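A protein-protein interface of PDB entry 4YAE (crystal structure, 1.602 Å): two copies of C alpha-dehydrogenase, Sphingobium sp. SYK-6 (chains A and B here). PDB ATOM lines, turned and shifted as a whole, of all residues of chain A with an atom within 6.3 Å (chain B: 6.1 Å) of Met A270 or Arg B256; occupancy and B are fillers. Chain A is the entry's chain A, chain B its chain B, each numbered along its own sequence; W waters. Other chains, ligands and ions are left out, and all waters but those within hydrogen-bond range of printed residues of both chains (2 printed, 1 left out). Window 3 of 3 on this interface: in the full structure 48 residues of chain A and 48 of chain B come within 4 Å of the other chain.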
ATOM      1  N   GLN A 264     -17.041  11.725 -24.318  1.00  0.00           N
ATOM      2  CA  GLN A 264     -18.333  12.333 -24.033  1.00  0.00           C
ATOM      3  C   GLN A 264     -18.225  13.365 -22.913  1.00  0.00           C
ATOM      4  O   GLN A 264     -18.843  14.424 -22.979  1.00  0.00           O
ATOM      5  CB  GLN A 264     -19.365  11.269 -23.654  1.00  0.00           C
ATOM      6  CG  GLN A 264     -20.789  11.816 -23.594  1.00  0.00           C
ATOM      7  CD  GLN A 264     -21.265  12.314 -24.946  1.00  0.00           C
ATOM      8  OE1 GLN A 264     -21.202  11.593 -25.941  1.00  0.00           O
ATOM      9  NE2 GLN A 264     -21.721  13.560 -24.991  1.00  0.00           N
ATOM     10  N   ALA A 265     -17.439  13.062 -21.885  1.00  0.00           N
ATOM     11  CA  ALA A 265     -17.262  13.998 -20.776  1.00  0.00           C
ATOM     12  C   ALA A 265     -16.584  15.277 -21.262  1.00  0.00           C
ATOM     13  O   ALA A 265     -16.931  16.374 -20.829  1.00  0.00           O
ATOM     14  CB  ALA A 265     -16.453  13.361 -19.659  1.00  0.00           C
ATOM     15  N   LEU A 266     -15.610  15.134 -22.156  1.00  0.00           N
ATOM     16  CA  LEU A 266     -14.948  16.289 -22.742  1.00  0.00           C
ATOM     17  C   LEU A 266     -15.956  17.137 -23.521  1.00  0.00           C
ATOM     18  O   LEU A 266     -16.021  18.354 -23.357  1.00  0.00           O
ATOM     19  CB  LEU A 266     -13.797  15.836 -23.645  1.00  0.00           C
ATOM     20  CG  LEU A 266     -12.563  15.316 -22.904  1.00  0.00           C
ATOM     21  CD1 LEU A 266     -11.676  14.486 -23.812  1.00  0.00           C
ATOM     22  CD2 LEU A 266     -11.759  16.482 -22.325  1.00  0.00           C
ATOM     23  N   LEU A 267     -16.751  16.485 -24.360  1.00  0.00           N
ATOM     24  CA  LEU A 267     -17.744  17.190 -25.161  1.00  0.00           C
ATOM     25  C   LEU A 267     -18.777  17.875 -24.277  1.00  0.00           C
ATOM     26  O   LEU A 267     -19.189  19.001 -24.559  1.00  0.00           O
ATOM     27  CB  LEU A 267     -18.431  16.224 -26.128  1.00  0.00           C
ATOM     28  CG  LEU A 267     -17.528  15.632 -27.206  1.00  0.00           C
ATOM     29  CD1 LEU A 267     -18.269  14.572 -28.010  1.00  0.00           C
ATOM     30  CD2 LEU A 267     -16.973  16.720 -28.123  1.00  0.00           C
ATOM     31  N   ASP A 268     -19.183  17.207 -23.203  1.00  0.00           N
ATOM     32  CA  ASP A 268     -20.214  17.756 -22.318  1.00  0.00           C
ATOM     33  C   ASP A 268     -19.736  19.025 -21.618  1.00  0.00           C
ATOM     34  O   ASP A 268     -20.551  19.843 -21.186  1.00  0.00           O
ATOM     35  CB  ASP A 268     -20.649  16.721 -21.271  1.00  0.00           C
ATOM     36  CG  ASP A 268     -21.436  15.559 -21.876  1.00  0.00           C
ATOM     37  OD1 ASP A 268     -21.913  15.675 -23.023  1.00  0.00           O
ATOM     38  OD2 ASP A 268     -21.579  14.519 -21.197  1.00  0.00           O
ATOM     39  N   SER A 269     -18.418  19.196 -21.511  1.00  0.00           N
ATOM     40  CA  SER A 269     -17.857  20.377 -20.852  1.00  0.00           C
ATOM     41  C   SER A 269     -17.948  21.621 -21.734  1.00  0.00           C
ATOM     42  O   SER A 269     -17.698  22.734 -21.279  1.00  0.00           O
ATOM     43  CB  SER A 269     -16.396  20.141 -20.454  1.00  0.00           C
ATOM     44  OG  SER A 269     -15.517  20.248 -21.565  1.00  0.00           O
ATOM     45  N   MET A 270     -18.312  21.431 -22.996  1.00  0.00           N
ATOM     46  CA  MET A 270     -18.300  22.518 -23.954  1.00  0.00           C
ATOM     47  C   MET A 270     -19.657  23.193 -23.973  1.00  0.00           C
ATOM     48  O   MET A 270     -20.676  22.514 -24.077  1.00  0.00           O
ATOM     49  CB  MET A 270     -17.943  21.998 -25.347  1.00  0.00           C
ATOM     50  CG  MET A 270     -16.555  21.386 -25.406  1.00  0.00           C
ATOM     51  SD  MET A 270     -16.137  20.714 -27.026  1.00  0.00           S
ATOM     52  CE  MET A 270     -14.614  19.866 -26.641  1.00  0.00           C
ATOM     53  N   PRO A 271     -19.679  24.531 -23.865  1.00  0.00           N
ATOM     54  CA  PRO A 271     -20.965  25.232 -23.914  1.00  0.00           C
ATOM     55  C   PRO A 271     -21.495  25.398 -25.332  1.00  0.00           C
ATOM     56  O   PRO A 271     -21.002  24.739 -26.245  1.00  0.00           O
ATOM     57  CB  PRO A 271     -20.639  26.592 -23.294  1.00  0.00           C
ATOM     58  CG  PRO A 271     -19.214  26.812 -23.630  1.00  0.00           C
ATOM     59  CD  PRO A 271     -18.565  25.454 -23.581  1.00  0.00           C
ATOM     60  N   LEU B 145      -8.115  24.272 -25.978  1.00  0.00           N
ATOM     61  CA  LEU B 145      -8.857  23.448 -26.932  1.00  0.00           C
ATOM     62  C   LEU B 145      -7.931  22.985 -28.051  1.00  0.00           C
ATOM     63  O   LEU B 145      -8.232  22.010 -28.734  1.00  0.00           O
ATOM     64  CB  LEU B 145     -10.056  24.206 -27.512  1.00  0.00           C
ATOM     65  CG  LEU B 145     -11.366  24.087 -26.729  1.00  0.00           C
ATOM     66  CD1 LEU B 145     -11.079  24.213 -25.348  1.00  0.00           C
ATOM     67  CD2 LEU B 145     -12.376  25.169 -27.094  1.00  0.00           C
ATOM     68  N   LEU B 148      -6.968  19.457 -27.992  1.00  0.00           N
ATOM     69  CA  LEU B 148      -8.063  18.513 -28.186  1.00  0.00           C
ATOM     70  C   LEU B 148      -8.547  18.427 -29.634  1.00  0.00           C
ATOM     71  O   LEU B 148      -8.730  17.333 -30.191  1.00  0.00           O
ATOM     72  CB  LEU B 148      -9.233  18.911 -27.285  1.00  0.00           C
ATOM     73  CG  LEU B 148     -10.105  17.819 -26.692  1.00  0.00           C
ATOM     74  CD1 LEU B 148      -9.296  16.788 -25.931  1.00  0.00           C
ATOM     75  CD2 LEU B 148     -11.117  18.500 -25.775  1.00  0.00           C
ATOM     76  N   SER B 250     -14.286  23.993 -20.441  1.00  0.00           N
ATOM     77  CA  SER B 250     -14.050  24.488 -21.791  1.00  0.00           C
ATOM     78  C   SER B 250     -14.748  25.824 -21.918  1.00  0.00           C
ATOM     79  O   SER B 250     -15.894  25.956 -21.503  1.00  0.00           O
ATOM     80  CB  SER B 250     -14.584  23.525 -22.843  1.00  0.00           C
ATOM     81  OG  SER B 250     -13.961  22.264 -22.734  1.00  0.00           O
ATOM     82  N   HIS B 252     -15.373  27.549 -24.785  1.00  0.00           N
ATOM     83  CA  HIS B 252     -16.044  27.719 -26.070  1.00  0.00           C
ATOM     84  C   HIS B 252     -16.579  26.386 -26.586  1.00  0.00           C
ATOM     85  O   HIS B 252     -15.972  25.339 -26.359  1.00  0.00           O
ATOM     86  CB  HIS B 252     -15.085  28.292 -27.125  1.00  0.00           C
ATOM     87  CG  HIS B 252     -14.784  29.749 -26.969  1.00  0.00           C
ATOM     88  ND1 HIS B 252     -13.858  30.229 -26.068  1.00  0.00           N
ATOM     89  CD2 HIS B 252     -15.263  30.831 -27.629  1.00  0.00           C
ATOM     90  CE1 HIS B 252     -13.790  31.544 -26.169  1.00  0.00           C
ATOM     91  NE2 HIS B 252     -14.634  31.935 -27.109  1.00  0.00           N
ATOM     92  N   GLY B 253     -17.695  26.433 -27.309  1.00  0.00           N
ATOM     93  CA  GLY B 253     -18.281  25.243 -27.909  1.00  0.00           C
ATOM     94  C   GLY B 253     -18.053  25.127 -29.406  1.00  0.00           C
ATOM     95  O   GLY B 253     -18.554  24.192 -30.043  1.00  0.00           O
ATOM     96  N   ASN B 254     -17.293  26.062 -29.970  1.00  0.00           N
ATOM     97  CA  ASN B 254     -17.130  26.157 -31.420  1.00  0.00           C
ATOM     98  C   ASN B 254     -16.410  24.962 -32.050  1.00  0.00           C
ATOM     99  O   ASN B 254     -16.505  24.750 -33.263  1.00  0.00           O
ATOM    100  CB  ASN B 254     -16.369  27.437 -31.778  1.00  0.00           C
ATOM    101  CG  ASN B 254     -17.003  28.676 -31.182  1.00  0.00           C
ATOM    102  OD1 ASN B 254     -16.986  28.872 -29.967  1.00  0.00           O
ATOM    103  ND2 ASN B 254     -17.565  29.522 -32.037  1.00  0.00           N
ATOM    104  N   TRP B 255     -15.697  24.191 -31.232  1.00  0.00           N
ATOM    105  CA  TRP B 255     -14.923  23.058 -31.729  1.00  0.00           C
ATOM    106  C   TRP B 255     -15.531  21.715 -31.318  1.00  0.00           C
ATOM    107  O   TRP B 255     -14.878  20.680 -31.393  1.00  0.00           O
ATOM    108  CB  TRP B 255     -13.468  23.192 -31.255  1.00  0.00           C
ATOM    109  CG  TRP B 255     -12.817  24.360 -31.925  1.00  0.00           C
ATOM    110  CD1 TRP B 255     -12.182  24.355 -33.133  1.00  0.00           C
ATOM    111  CD2 TRP B 255     -12.786  25.718 -31.461  1.00  0.00           C
ATOM    112  NE1 TRP B 255     -11.746  25.620 -33.445  1.00  0.00           N
ATOM    113  CE2 TRP B 255     -12.101  26.475 -32.434  1.00  0.00           C
ATOM    114  CE3 TRP B 255     -13.265  26.364 -30.315  1.00  0.00           C
ATOM    115  CZ2 TRP B 255     -11.877  27.846 -32.293  1.00  0.00           C
ATOM    116  CZ3 TRP B 255     -13.041  27.730 -30.177  1.00  0.00           C
ATOM    117  CH2 TRP B 255     -12.355  28.454 -31.161  1.00  0.00           C
ATOM    118  N   ARG B 256     -16.802  21.729 -30.929  1.00  0.00           N
ATOM    119  CA  ARG B 256     -17.504  20.493 -30.593  1.00  0.00           C
ATOM    120  C   ARG B 256     -17.497  19.490 -31.747  1.00  0.00           C
ATOM    121  O   ARG B 256     -17.137  18.334 -31.558  1.00  0.00           O
ATOM    122  CB  ARG B 256     -18.951  20.789 -30.194  1.00  0.00           C
ATOM    123  CG  ARG B 256     -19.795  19.540 -29.965  1.00  0.00           C
ATOM    124  CD  ARG B 256     -21.220  19.899 -29.553  1.00  0.00           C
ATOM    125  NE  ARG B 256     -21.235  20.603 -28.275  1.00  0.00           N
ATOM    126  CZ  ARG B 256     -21.274  20.005 -27.088  1.00  0.00           C
ATOM    127  NH1 ARG B 256     -21.318  18.682 -26.998  1.00  0.00           N
ATOM    128  NH2 ARG B 256     -21.283  20.736 -25.984  1.00  0.00           N
ATOM    129  N   GLU B 257     -17.914  19.936 -32.931  1.00  0.00           N
ATOM    130  CA  GLU B 257     -18.032  19.050 -34.084  1.00  0.00           C
ATOM    131  C   GLU B 257     -16.666  18.560 -34.559  1.00  0.00           C
ATOM    132  O   GLU B 257     -16.531  17.408 -34.968  1.00  0.00           O
ATOM    133  CB  GLU B 257     -18.761  19.754 -35.234  1.00  0.00           C
ATOM    134  CG  GLU B 257     -20.090  20.378 -34.840  1.00  0.00           C
ATOM    135  CD  GLU B 257     -21.033  19.388 -34.190  1.00  0.00           C
ATOM    136  OE1 GLU B 257     -21.004  18.200 -34.577  1.00  0.00           O
ATOM    137  OE2 GLU B 257     -21.800  19.797 -33.292  1.00  0.00           O
ATOM    138  N   THR B 258     -15.654  19.425 -34.501  1.00  0.00           N
ATOM    139  CA  THR B 258     -14.325  19.037 -34.975  1.00  0.00           C
ATOM    140  C   THR B 258     -13.694  18.048 -34.005  1.00  0.00           C
ATOM    141  O   THR B 258     -13.003  17.113 -34.427  1.00  0.00           O
ATOM    142  CB  THR B 258     -13.400  20.260 -35.170  1.00  0.00           C
ATOM    143  OG1 THR B 258     -13.457  21.112 -34.020  1.00  0.00           O
ATOM    144  CG2 THR B 258     -13.822  21.046 -36.407  1.00  0.00           C
ATOM    145  N   CYS B 259     -13.952  18.227 -32.713  1.00  0.00           N
ATOM    146  CA  CYS B 259     -13.500  17.257 -31.726  1.00  0.00           C
ATOM    147  C   CYS B 259     -14.242  15.942 -31.924  1.00  0.00           C
ATOM    148  O   CYS B 259     -13.629  14.886 -31.914  1.00  0.00           O
ATOM    149  CB  CYS B 259     -13.702  17.771 -30.304  1.00  0.00           C
ATOM    150  SG  CYS B 259     -12.513  19.025 -29.808  1.00  0.00           S
ATOM    151  N   GLU B 260     -15.559  16.006 -32.115  1.00  0.00           N
ATOM    152  CA  GLU B 260     -16.333  14.790 -32.341  1.00  0.00           C
ATOM    153  C   GLU B 260     -15.789  13.966 -33.509  1.00  0.00           C
ATOM    154  O   GLU B 260     -15.730  12.739 -33.437  1.00  0.00           O
ATOM    155  CB  GLU B 260     -17.811  15.129 -32.594  1.00  0.00           C
ATOM    156  CG  GLU B 260     -18.612  15.285 -31.323  1.00  0.00           C
ATOM    157  CD  GLU B 260     -20.083  15.561 -31.580  1.00  0.00           C
ATOM    158  OE1 GLU B 260     -20.408  16.147 -32.633  1.00  0.00           O
ATOM    159  OE2 GLU B 260     -20.913  15.189 -30.726  1.00  0.00           O
ATOM    160  N   ALA B 261     -15.375  14.641 -34.575  1.00  0.00           N
ATOM    161  CA  ALA B 261     -14.877  13.957 -35.762  1.00  0.00           C
ATOM    162  C   ALA B 261     -13.550  13.272 -35.464  1.00  0.00           C
ATOM    163  O   ALA B 261     -13.318  12.142 -35.883  1.00  0.00           O
ATOM    164  CB  ALA B 261     -14.722  14.933 -36.919  1.00  0.00           C
ATOM    165  N   PHE B 263     -12.545  12.320 -32.448  1.00  0.00           N
ATOM    166  CA  PHE B 263     -12.832  11.255 -31.501  1.00  0.00           C
ATOM    167  C   PHE B 263     -13.371  10.055 -32.258  1.00  0.00           C
ATOM    168  O   PHE B 263     -13.008   8.914 -31.975  1.00  0.00           O
ATOM    169  CB  PHE B 263     -13.837  11.715 -30.440  1.00  0.00           C
ATOM    170  CG  PHE B 263     -13.315  12.787 -29.507  1.00  0.00           C
ATOM    171  CD1 PHE B 263     -11.954  13.001 -29.329  1.00  0.00           C
ATOM    172  CD2 PHE B 263     -14.201  13.583 -28.805  1.00  0.00           C
ATOM    173  CE1 PHE B 263     -11.501  13.982 -28.460  1.00  0.00           C
ATOM    174  CE2 PHE B 263     -13.751  14.560 -27.938  1.00  0.00           C
ATOM    175  CZ  PHE B 263     -12.401  14.763 -27.771  1.00  0.00           C
HETATM  176  O   HOH W   1     -22.222  17.207 -25.310  1.00  0.00           O
HETATM  177  O   HOH W   2     -17.080  23.779 -19.077  1.00  0.00           O
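O of Met A270 sits at hydrogen-bond distance from NH2 of Arg B256.
OG of Ser B250 lies within hydrogen-bond range of OG of Ser A269 (2.8 Å).
The backbone carbonyl oxygen (O) of Leu A267 sits at hydrogen-bond distance from the guanidinium group (NH2) of Arg B256.
The side-chain hydroxyl (OG) of Ser A269 sits at hydrogen-bond distance from the backbone carbonyl oxygen (O) of Leu A266, at 2.7 Å.
The backbone carbonyl oxygen (O) of Trp B255 sits at hydrogen-bond distance from the side-chain sulfur (SG) of Cys B259 (3.3 Å).
Among the printed residues, merely in contact across the chains: Leu A266 with Leu B148 (3.9 Å), Leu A267 with Glu B260 (3.4 Å), Leu A267 with Phe B263 (3.9 Å), Met A270 with Leu B148 (3.9 Å), Met A270 with Ser B250 (3.8 Å), Met A270 with Cys B259 (3.9 Å), Pro A271 with Ser B250 (3.4 Å), Pro A271 with His B252 (3.7 Å) and Pro A271 with Gly B253 (3.2 Å).
Printed residues of chain B within 4 Å of Met A270: Leu B148 (3.9 Å), Ser B250 (3.8 Å), Arg B256 (2.7 Å) and Cys B259 (3.9 Å).
Of the printed residues of chain A, Ser B250 touches Ser A269 (2.8 Å), Met A270 (3.8 Å) and Pro A271 (3.4 Å).
Of the printed residues of chain A, His B252 touches Pro A271 (3.7 Å).
Printed residues of chain A within 4 Å of Gly B253: Pro A271.
Leu B145 touches none of the printed residues of chain A.
The nearest residue of chain A that does not touch Arg B256 is Pro A271 (4.02 Å).
Of the 14 printed residues of chain B, 8 touch a printed residue of chain A.
Along chain B the printed residues that touch a printed residue of chain A span positions 148 to 263.
Of the 8 printed residues of chain A, 5 touch a printed residue of chain B.
No position is printed for both chains.
Of the 12 pairs that touch across the chains among the printed residues, none has its exchanged pair printed and touching as well.
Water W1 bridges NH1 of Arg B256 and OD1 of Asp A268.
Water W2 bridges O of Ser A269 (2.5 Å) and N of Ser B250 (3.1 Å).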
